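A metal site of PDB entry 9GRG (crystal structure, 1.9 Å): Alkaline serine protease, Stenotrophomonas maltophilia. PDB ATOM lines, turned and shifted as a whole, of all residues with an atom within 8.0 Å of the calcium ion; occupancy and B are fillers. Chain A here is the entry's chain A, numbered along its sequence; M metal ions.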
ATOM      1  N   PRO A   3       1.866  12.897  20.277  1.00  0.00           N
ATOM      2  CA  PRO A   3       2.232  13.549  19.021  1.00  0.00           C
ATOM      3  C   PRO A   3       1.959  12.583  17.869  1.00  0.00           C
ATOM      4  O   PRO A   3       1.880  11.383  18.101  1.00  0.00           O
ATOM      5  CB  PRO A   3       3.755  13.794  19.248  1.00  0.00           C
ATOM      6  CG  PRO A   3       4.167  12.625  20.111  1.00  0.00           C
ATOM      7  CD  PRO A   3       3.024  12.567  21.140  1.00  0.00           C
ATOM      8  N   ASN A   4       1.903  13.100  16.630  1.00  0.00           N
ATOM      9  CA  ASN A   4       1.504  12.309  15.470  1.00  0.00           C
ATOM     10  C   ASN A   4       2.703  11.757  14.694  1.00  0.00           C
ATOM     11  O   ASN A   4       2.570  11.248  13.581  1.00  0.00           O
ATOM     12  CB  ASN A   4       0.606  13.115  14.527  1.00  0.00           C
ATOM     13  CG  ASN A   4       1.400  14.216  13.887  1.00  0.00           C
ATOM     14  OD1 ASN A   4       2.608  14.334  14.132  1.00  0.00           O
ATOM     15  ND2 ASN A   4       0.743  15.078  13.127  1.00  0.00           N
ATOM     16  N   ASP A   5       3.908  11.840  15.260  1.00  0.00           N
ATOM     17  CA  ASP A   5       5.063  11.280  14.554  1.00  0.00           C
ATOM     18  C   ASP A   5       4.827   9.810  14.259  1.00  0.00           C
ATOM     19  O   ASP A   5       4.567   9.012  15.174  1.00  0.00           O
ATOM     20  CB  ASP A   5       6.356  11.554  15.324  1.00  0.00           C
ATOM     21  CG  ASP A   5       6.510  12.995  15.801  1.00  0.00           C
ATOM     22  OD1 ASP A   5       5.873  13.345  16.826  1.00  0.00           O
ATOM     23  OD2 ASP A   5       7.209  13.766  15.118  1.00  0.00           O
ATOM     24  N   PRO A   6       4.958   9.398  12.983  1.00  0.00           N
ATOM     25  CA  PRO A   6       4.557   8.061  12.560  1.00  0.00           C
ATOM     26  C   PRO A   6       5.198   6.910  13.325  1.00  0.00           C
ATOM     27  O   PRO A   6       4.523   5.914  13.550  1.00  0.00           O
ATOM     28  CB  PRO A   6       4.847   7.959  11.061  1.00  0.00           C
ATOM     29  CG  PRO A   6       5.523   9.277  10.725  1.00  0.00           C
ATOM     30  CD  PRO A   6       5.395  10.243  11.864  1.00  0.00           C
ATOM     31  N   TYR A   7       6.492   7.025  13.690  1.00  0.00           N
ATOM     32  CA  TYR A   7       7.181   5.906  14.326  1.00  0.00           C
ATOM     33  C   TYR A   7       7.155   5.977  15.858  1.00  0.00           C
ATOM     34  O   TYR A   7       7.676   5.070  16.510  1.00  0.00           O
ATOM     35  CB  TYR A   7       8.644   5.917  13.838  1.00  0.00           C
ATOM     36  CG  TYR A   7       8.807   5.548  12.377  1.00  0.00           C
ATOM     37  CD1 TYR A   7       7.973   4.604  11.785  1.00  0.00           C
ATOM     38  CD2 TYR A   7       9.800   6.112  11.601  1.00  0.00           C
ATOM     39  CE1 TYR A   7       8.120   4.243  10.457  1.00  0.00           C
ATOM     40  CE2 TYR A   7       9.971   5.737  10.289  1.00  0.00           C
ATOM     41  CZ  TYR A   7       9.120   4.832   9.706  1.00  0.00           C
ATOM     42  OH  TYR A   7       9.254   4.452   8.393  1.00  0.00           O
ATOM     43  N   TYR A   8       6.597   7.052  16.419  1.00  0.00           N
ATOM     44  CA  TYR A   8       6.653   7.301  17.858  1.00  0.00           C
ATOM     45  C   TYR A   8       6.014   6.176  18.667  1.00  0.00           C
ATOM     46  O   TYR A   8       6.605   5.661  19.656  1.00  0.00           O
ATOM     47  CB  TYR A   8       5.975   8.644  18.162  1.00  0.00           C
ATOM     48  CG  TYR A   8       5.537   8.876  19.600  1.00  0.00           C
ATOM     49  CD1 TYR A   8       6.454   9.239  20.593  1.00  0.00           C
ATOM     50  CD2 TYR A   8       4.193   8.810  19.949  1.00  0.00           C
ATOM     51  CE1 TYR A   8       6.033   9.508  21.893  1.00  0.00           C
ATOM     52  CE2 TYR A   8       3.767   9.086  21.238  1.00  0.00           C
ATOM     53  CZ  TYR A   8       4.687   9.405  22.217  1.00  0.00           C
ATOM     54  OH  TYR A   8       4.232   9.596  23.488  1.00  0.00           O
ATOM     55  N   GLN A  12       9.050   4.287  20.270  1.00  0.00           N
ATOM     56  CA  GLN A  12       9.663   5.137  21.291  1.00  0.00           C
ATOM     57  C   GLN A  12       9.154   4.854  22.703  1.00  0.00           C
ATOM     58  O   GLN A  12       8.731   5.755  23.432  1.00  0.00           O
ATOM     59  CB  GLN A  12       9.768   6.615  20.939  1.00  0.00           C
ATOM     60  CG  GLN A  12      10.471   6.842  19.610  1.00  0.00           C
ATOM     61  CD  GLN A  12      10.567   8.310  19.318  1.00  0.00           C
ATOM     62  OE1 GLN A  12       9.535   8.967  19.043  1.00  0.00           O
ATOM     63  NE2 GLN A  12      11.780   8.848  19.412  1.00  0.00           N
ATOM     64  N   HIS A  49      19.005  17.091   8.545  1.00  0.00           N
ATOM     65  CA  HIS A  49      18.106  15.961   8.731  1.00  0.00           C
ATOM     66  C   HIS A  49      16.689  16.545   8.795  1.00  0.00           C
ATOM     67  O   HIS A  49      16.465  17.483   9.545  1.00  0.00           O
ATOM     68  CB  HIS A  49      18.411  15.198  10.027  1.00  0.00           C
ATOM     69  CG  HIS A  49      17.675  13.885  10.094  1.00  0.00           C
ATOM     70  ND1 HIS A  49      16.303  13.821  10.173  1.00  0.00           N
ATOM     71  CD2 HIS A  49      18.118  12.595  10.020  1.00  0.00           C
ATOM     72  CE1 HIS A  49      15.925  12.538  10.213  1.00  0.00           C
ATOM     73  NE2 HIS A  49      17.012  11.769  10.104  1.00  0.00           N
ATOM     74  N   PRO A  50      15.719  16.058   7.992  1.00  0.00           N
ATOM     75  CA  PRO A  50      14.413  16.726   7.920  1.00  0.00           C
ATOM     76  C   PRO A  50      13.599  16.633   9.190  1.00  0.00           C
ATOM     77  O   PRO A  50      12.642  17.385   9.346  1.00  0.00           O
ATOM     78  CB  PRO A  50      13.711  16.050   6.735  1.00  0.00           C
ATOM     79  CG  PRO A  50      14.375  14.669   6.696  1.00  0.00           C
ATOM     80  CD  PRO A  50      15.834  14.922   7.062  1.00  0.00           C
ATOM     81  N   ASP A  51      14.000  15.758  10.124  1.00  0.00           N
ATOM     82  CA  ASP A  51      13.309  15.728  11.406  1.00  0.00           C
ATOM     83  C   ASP A  51      13.993  16.586  12.489  1.00  0.00           C
ATOM     84  O   ASP A  51      13.550  16.552  13.644  1.00  0.00           O
ATOM     85  CB  ASP A  51      12.998  14.329  11.924  1.00  0.00           C
ATOM     86  CG  ASP A  51      11.679  14.244  12.709  1.00  0.00           C
ATOM     87  OD1 ASP A  51      10.767  15.135  12.454  1.00  0.00           O
ATOM     88  OD2 ASP A  51      11.530  13.312  13.590  1.00  0.00           O
ATOM     89  N   LEU A  52      15.109  17.269  12.140  1.00  0.00           N
ATOM     90  CA  LEU A  52      15.832  18.149  13.060  1.00  0.00           C
ATOM     91  C   LEU A  52      15.801  19.613  12.615  1.00  0.00           C
ATOM     92  O   LEU A  52      15.908  20.496  13.457  1.00  0.00           O
ATOM     93  CB  LEU A  52      17.296  17.713  13.131  1.00  0.00           C
ATOM     94  CG  LEU A  52      17.579  16.361  13.789  1.00  0.00           C
ATOM     95  CD1 LEU A  52      19.117  16.182  13.827  1.00  0.00           C
ATOM     96  CD2 LEU A  52      17.007  16.266  15.203  1.00  0.00           C
ATOM     97  N   ALA A 114      15.935  17.102  20.998  1.00  0.00           N
ATOM     98  CA  ALA A 114      14.988  18.052  20.434  1.00  0.00           C
ATOM     99  C   ALA A 114      14.521  17.658  19.036  1.00  0.00           C
ATOM    100  O   ALA A 114      14.255  18.533  18.215  1.00  0.00           O
ATOM    101  CB  ALA A 114      15.577  19.464  20.429  1.00  0.00           C
ATOM    102  N   GLU A 115      14.380  16.347  18.745  1.00  0.00           N
ATOM    103  CA  GLU A 115      13.845  15.981  17.455  1.00  0.00           C
ATOM    104  C   GLU A 115      12.498  16.696  17.271  1.00  0.00           C
ATOM    105  O   GLU A 115      11.724  16.754  18.223  1.00  0.00           O
ATOM    106  CB  GLU A 115      13.654  14.464  17.399  1.00  0.00           C
ATOM    107  CG  GLU A 115      13.218  13.983  16.021  1.00  0.00           C
ATOM    108  CD  GLU A 115      13.798  12.646  15.605  1.00  0.00           C
ATOM    109  OE1 GLU A 115      14.667  12.160  16.364  1.00  0.00           O
ATOM    110  OE2 GLU A 115      13.418  12.121  14.522  1.00  0.00           O
ATOM    111  N   GLN A 116      12.241  17.198  16.065  1.00  0.00           N
ATOM    112  CA  GLN A 116      10.952  17.858  15.809  1.00  0.00           C
ATOM    113  C   GLN A 116       9.816  16.856  16.064  1.00  0.00           C
ATOM    114  O   GLN A 116       9.831  15.719  15.555  1.00  0.00           O
ATOM    115  CB  GLN A 116      10.914  18.309  14.347  1.00  0.00           C
ATOM    116  CG  GLN A 116      11.825  19.483  14.013  1.00  0.00           C
ATOM    117  CD  GLN A 116      11.164  20.817  14.321  1.00  0.00           C
ATOM    118  OE1 GLN A 116      10.221  20.850  15.104  1.00  0.00           O
ATOM    119  NE2 GLN A 116      11.667  21.901  13.750  1.00  0.00           N
ATOM    120  N   THR A 117       8.802  17.307  16.810  1.00  0.00           N
ATOM    121  CA  THR A 117       7.740  16.432  17.279  1.00  0.00           C
ATOM    122  C   THR A 117       6.379  16.981  16.832  1.00  0.00           C
ATOM    123  O   THR A 117       6.211  18.187  16.632  1.00  0.00           O
ATOM    124  CB  THR A 117       7.891  16.331  18.802  1.00  0.00           C
ATOM    125  OG1 THR A 117       9.180  15.715  19.064  1.00  0.00           O
ATOM    126  CG2 THR A 117       6.801  15.474  19.434  1.00  0.00           C
ATOM    127  N   ASN A 118       5.431  16.070  16.597  1.00  0.00           N
ATOM    128  CA  ASN A 118       4.068  16.409  16.178  1.00  0.00           C
ATOM    129  C   ASN A 118       4.071  17.030  14.779  1.00  0.00           C
ATOM    130  O   ASN A 118       3.122  17.731  14.398  1.00  0.00           O
ATOM    131  CB  ASN A 118       3.339  17.152  17.303  1.00  0.00           C
ATOM    132  CG  ASN A 118       1.848  16.998  17.148  1.00  0.00           C
ATOM    133  OD1 ASN A 118       1.356  15.905  16.872  1.00  0.00           O
ATOM    134  ND2 ASN A 118       1.129  18.106  17.246  1.00  0.00           N
ATOM    135  N   ASN A 119       5.107  16.685  13.979  1.00  0.00           N
ATOM    136  CA  ASN A 119       5.324  17.242  12.657  1.00  0.00           C
ATOM    137  C   ASN A 119       5.012  16.210  11.570  1.00  0.00           C
ATOM    138  O   ASN A 119       5.303  16.433  10.401  1.00  0.00           O
ATOM    139  CB  ASN A 119       6.707  17.877  12.539  1.00  0.00           C
ATOM    140  CG  ASN A 119       7.789  16.823  12.450  1.00  0.00           C
ATOM    141  OD1 ASN A 119       7.619  15.731  13.013  1.00  0.00           O
ATOM    142  ND2 ASN A 119       8.910  17.124  11.808  1.00  0.00           N
ATOM    143  N   GLY A 120       4.403  15.071  11.924  1.00  0.00           N
ATOM    144  CA  GLY A 120       4.005  14.122  10.894  1.00  0.00           C
ATOM    145  C   GLY A 120       5.205  13.442  10.220  1.00  0.00           C
ATOM    146  O   GLY A 120       5.067  12.924   9.105  1.00  0.00           O
ATOM    147  N   VAL A 121       6.353  13.423  10.894  1.00  0.00           N
ATOM    148  CA  VAL A 121       7.601  12.952  10.289  1.00  0.00           C
ATOM    149  C   VAL A 121       8.390  12.190  11.351  1.00  0.00           C
ATOM    150  O   VAL A 121       8.650  12.682  12.426  1.00  0.00           O
ATOM    151  CB  VAL A 121       8.496  14.071   9.702  1.00  0.00           C
ATOM    152  CG1 VAL A 121       9.821  13.491   9.160  1.00  0.00           C
ATOM    153  CG2 VAL A 121       7.839  14.819   8.541  1.00  0.00           C
ATOM    154  N   GLY A 122       8.786  10.962  11.028  1.00  0.00           N
ATOM    155  CA  GLY A 122       9.820  10.322  11.820  1.00  0.00           C
ATOM    156  C   GLY A 122       9.410  10.019  13.259  1.00  0.00           C
ATOM    157  O   GLY A 122       8.439   9.311  13.523  1.00  0.00           O
ATOM    158  N   MET A 123      10.296  10.462  14.169  1.00  0.00           N
ATOM    159  CA  MET A 123      10.207  10.163  15.578  1.00  0.00           C
ATOM    160  C   MET A 123       9.929  11.463  16.341  1.00  0.00           C
ATOM    161  O   MET A 123       9.909  12.552  15.742  1.00  0.00           O
ATOM    162  CB  MET A 123      11.579   9.647  16.053  1.00  0.00           C
ATOM    163  CG  MET A 123      12.107   8.452  15.301  1.00  0.00           C
ATOM    164  SD  MET A 123      11.410   6.937  15.966  1.00  0.00           S
ATOM    165  CE  MET A 123      12.012   5.652  14.849  1.00  0.00           C
ATOM    166  N   ALA A 124       9.754  11.330  17.659  1.00  0.00           N
ATOM    167  CA  ALA A 124       9.619  12.460  18.562  1.00  0.00           C
ATOM    168  C   ALA A 124      10.937  12.691  19.324  1.00  0.00           C
ATOM    169  O   ALA A 124      11.849  11.841  19.280  1.00  0.00           O
ATOM    170  CB  ALA A 124       8.503  12.143  19.528  1.00  0.00           C
ATOM    171  N   GLY A 125      11.063  13.889  19.913  1.00  0.00           N
ATOM    172  CA  GLY A 125      12.147  14.287  20.813  1.00  0.00           C
ATOM    173  C   GLY A 125      11.577  14.857  22.102  1.00  0.00           C
ATOM    174  O   GLY A 125      10.424  15.298  22.145  1.00  0.00           O
ATOM    175  N   HIS A 128      11.419  19.244  22.487  1.00  0.00           N
ATOM    176  CA  HIS A 128      11.260  19.408  21.042  1.00  0.00           C
ATOM    177  C   HIS A 128      10.908  20.846  20.625  1.00  0.00           C
ATOM    178  O   HIS A 128      10.773  21.098  19.417  1.00  0.00           O
ATOM    179  CB  HIS A 128      10.275  18.392  20.481  1.00  0.00           C
ATOM    180  CG  HIS A 128       8.943  18.348  21.172  1.00  0.00           C
ATOM    181  ND1 HIS A 128       8.524  17.312  21.982  1.00  0.00           N
ATOM    182  CD2 HIS A 128       7.893  19.192  21.048  1.00  0.00           C
ATOM    183  CE1 HIS A 128       7.279  17.555  22.406  1.00  0.00           C
ATOM    184  NE2 HIS A 128       6.867  18.683  21.842  1.00  0.00           N
ATOM    185  N   TYR A 282      16.177   6.728  10.580  1.00  0.00           N
ATOM    186  CA  TYR A 282      15.975   6.666  12.024  1.00  0.00           C
ATOM    187  C   TYR A 282      16.754   5.452  12.508  1.00  0.00           C
ATOM    188  O   TYR A 282      16.660   4.406  11.883  1.00  0.00           O
ATOM    189  CB  TYR A 282      14.473   6.645  12.310  1.00  0.00           C
ATOM    190  CG  TYR A 282      13.856   7.885  11.688  1.00  0.00           C
ATOM    191  CD1 TYR A 282      13.901   9.115  12.350  1.00  0.00           C
ATOM    192  CD2 TYR A 282      13.351   7.880  10.394  1.00  0.00           C
ATOM    193  CE1 TYR A 282      13.407  10.276  11.766  1.00  0.00           C
ATOM    194  CE2 TYR A 282      12.824   9.023   9.808  1.00  0.00           C
ATOM    195  CZ  TYR A 282      12.864  10.229  10.488  1.00  0.00           C
ATOM    196  OH  TYR A 282      12.387  11.395   9.941  1.00  0.00           O
HETATM  197 CA    CA M   1       9.193  14.129  14.005  1.00  0.00          CA
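A ring nitrogen (ND1) of His 49 sits at hydrogen-bond distance from the backbone NH of Asp 51, at 3.0 Å.
The side-chain amide oxygen (OD1) of Asn 4 is in hydrogen-bond range of the backbone NH (N) of Asn 119 (3.4 Å).
OD2 of Asp 51 sits close to OE2 of Glu 115 (2.4 Å).
N of Asn 118 is in hydrogen-bond range of OD1 of Asp 5, 2.8 Å away.
Within 4 Å of the calcium ion: Asp 5, Asp 51, Gln 116, Asn 119, Val 121 and Met 123.
The nearest printed residue that does not touch the calcium ion is Gly 122 (4.2 Å).
The calcium ion is bound by O of Val 121 (2.2 Å), OD2 of Asp 5 (2.3 Å), O of Gln 116 (2.3 Å), OD1 of Asp 51 (2.4 Å), O of Met 123 (2.5 Å), OD1 of Asn 119 (2.5 Å) and OD2 of Asp 51 (2.5 Å).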
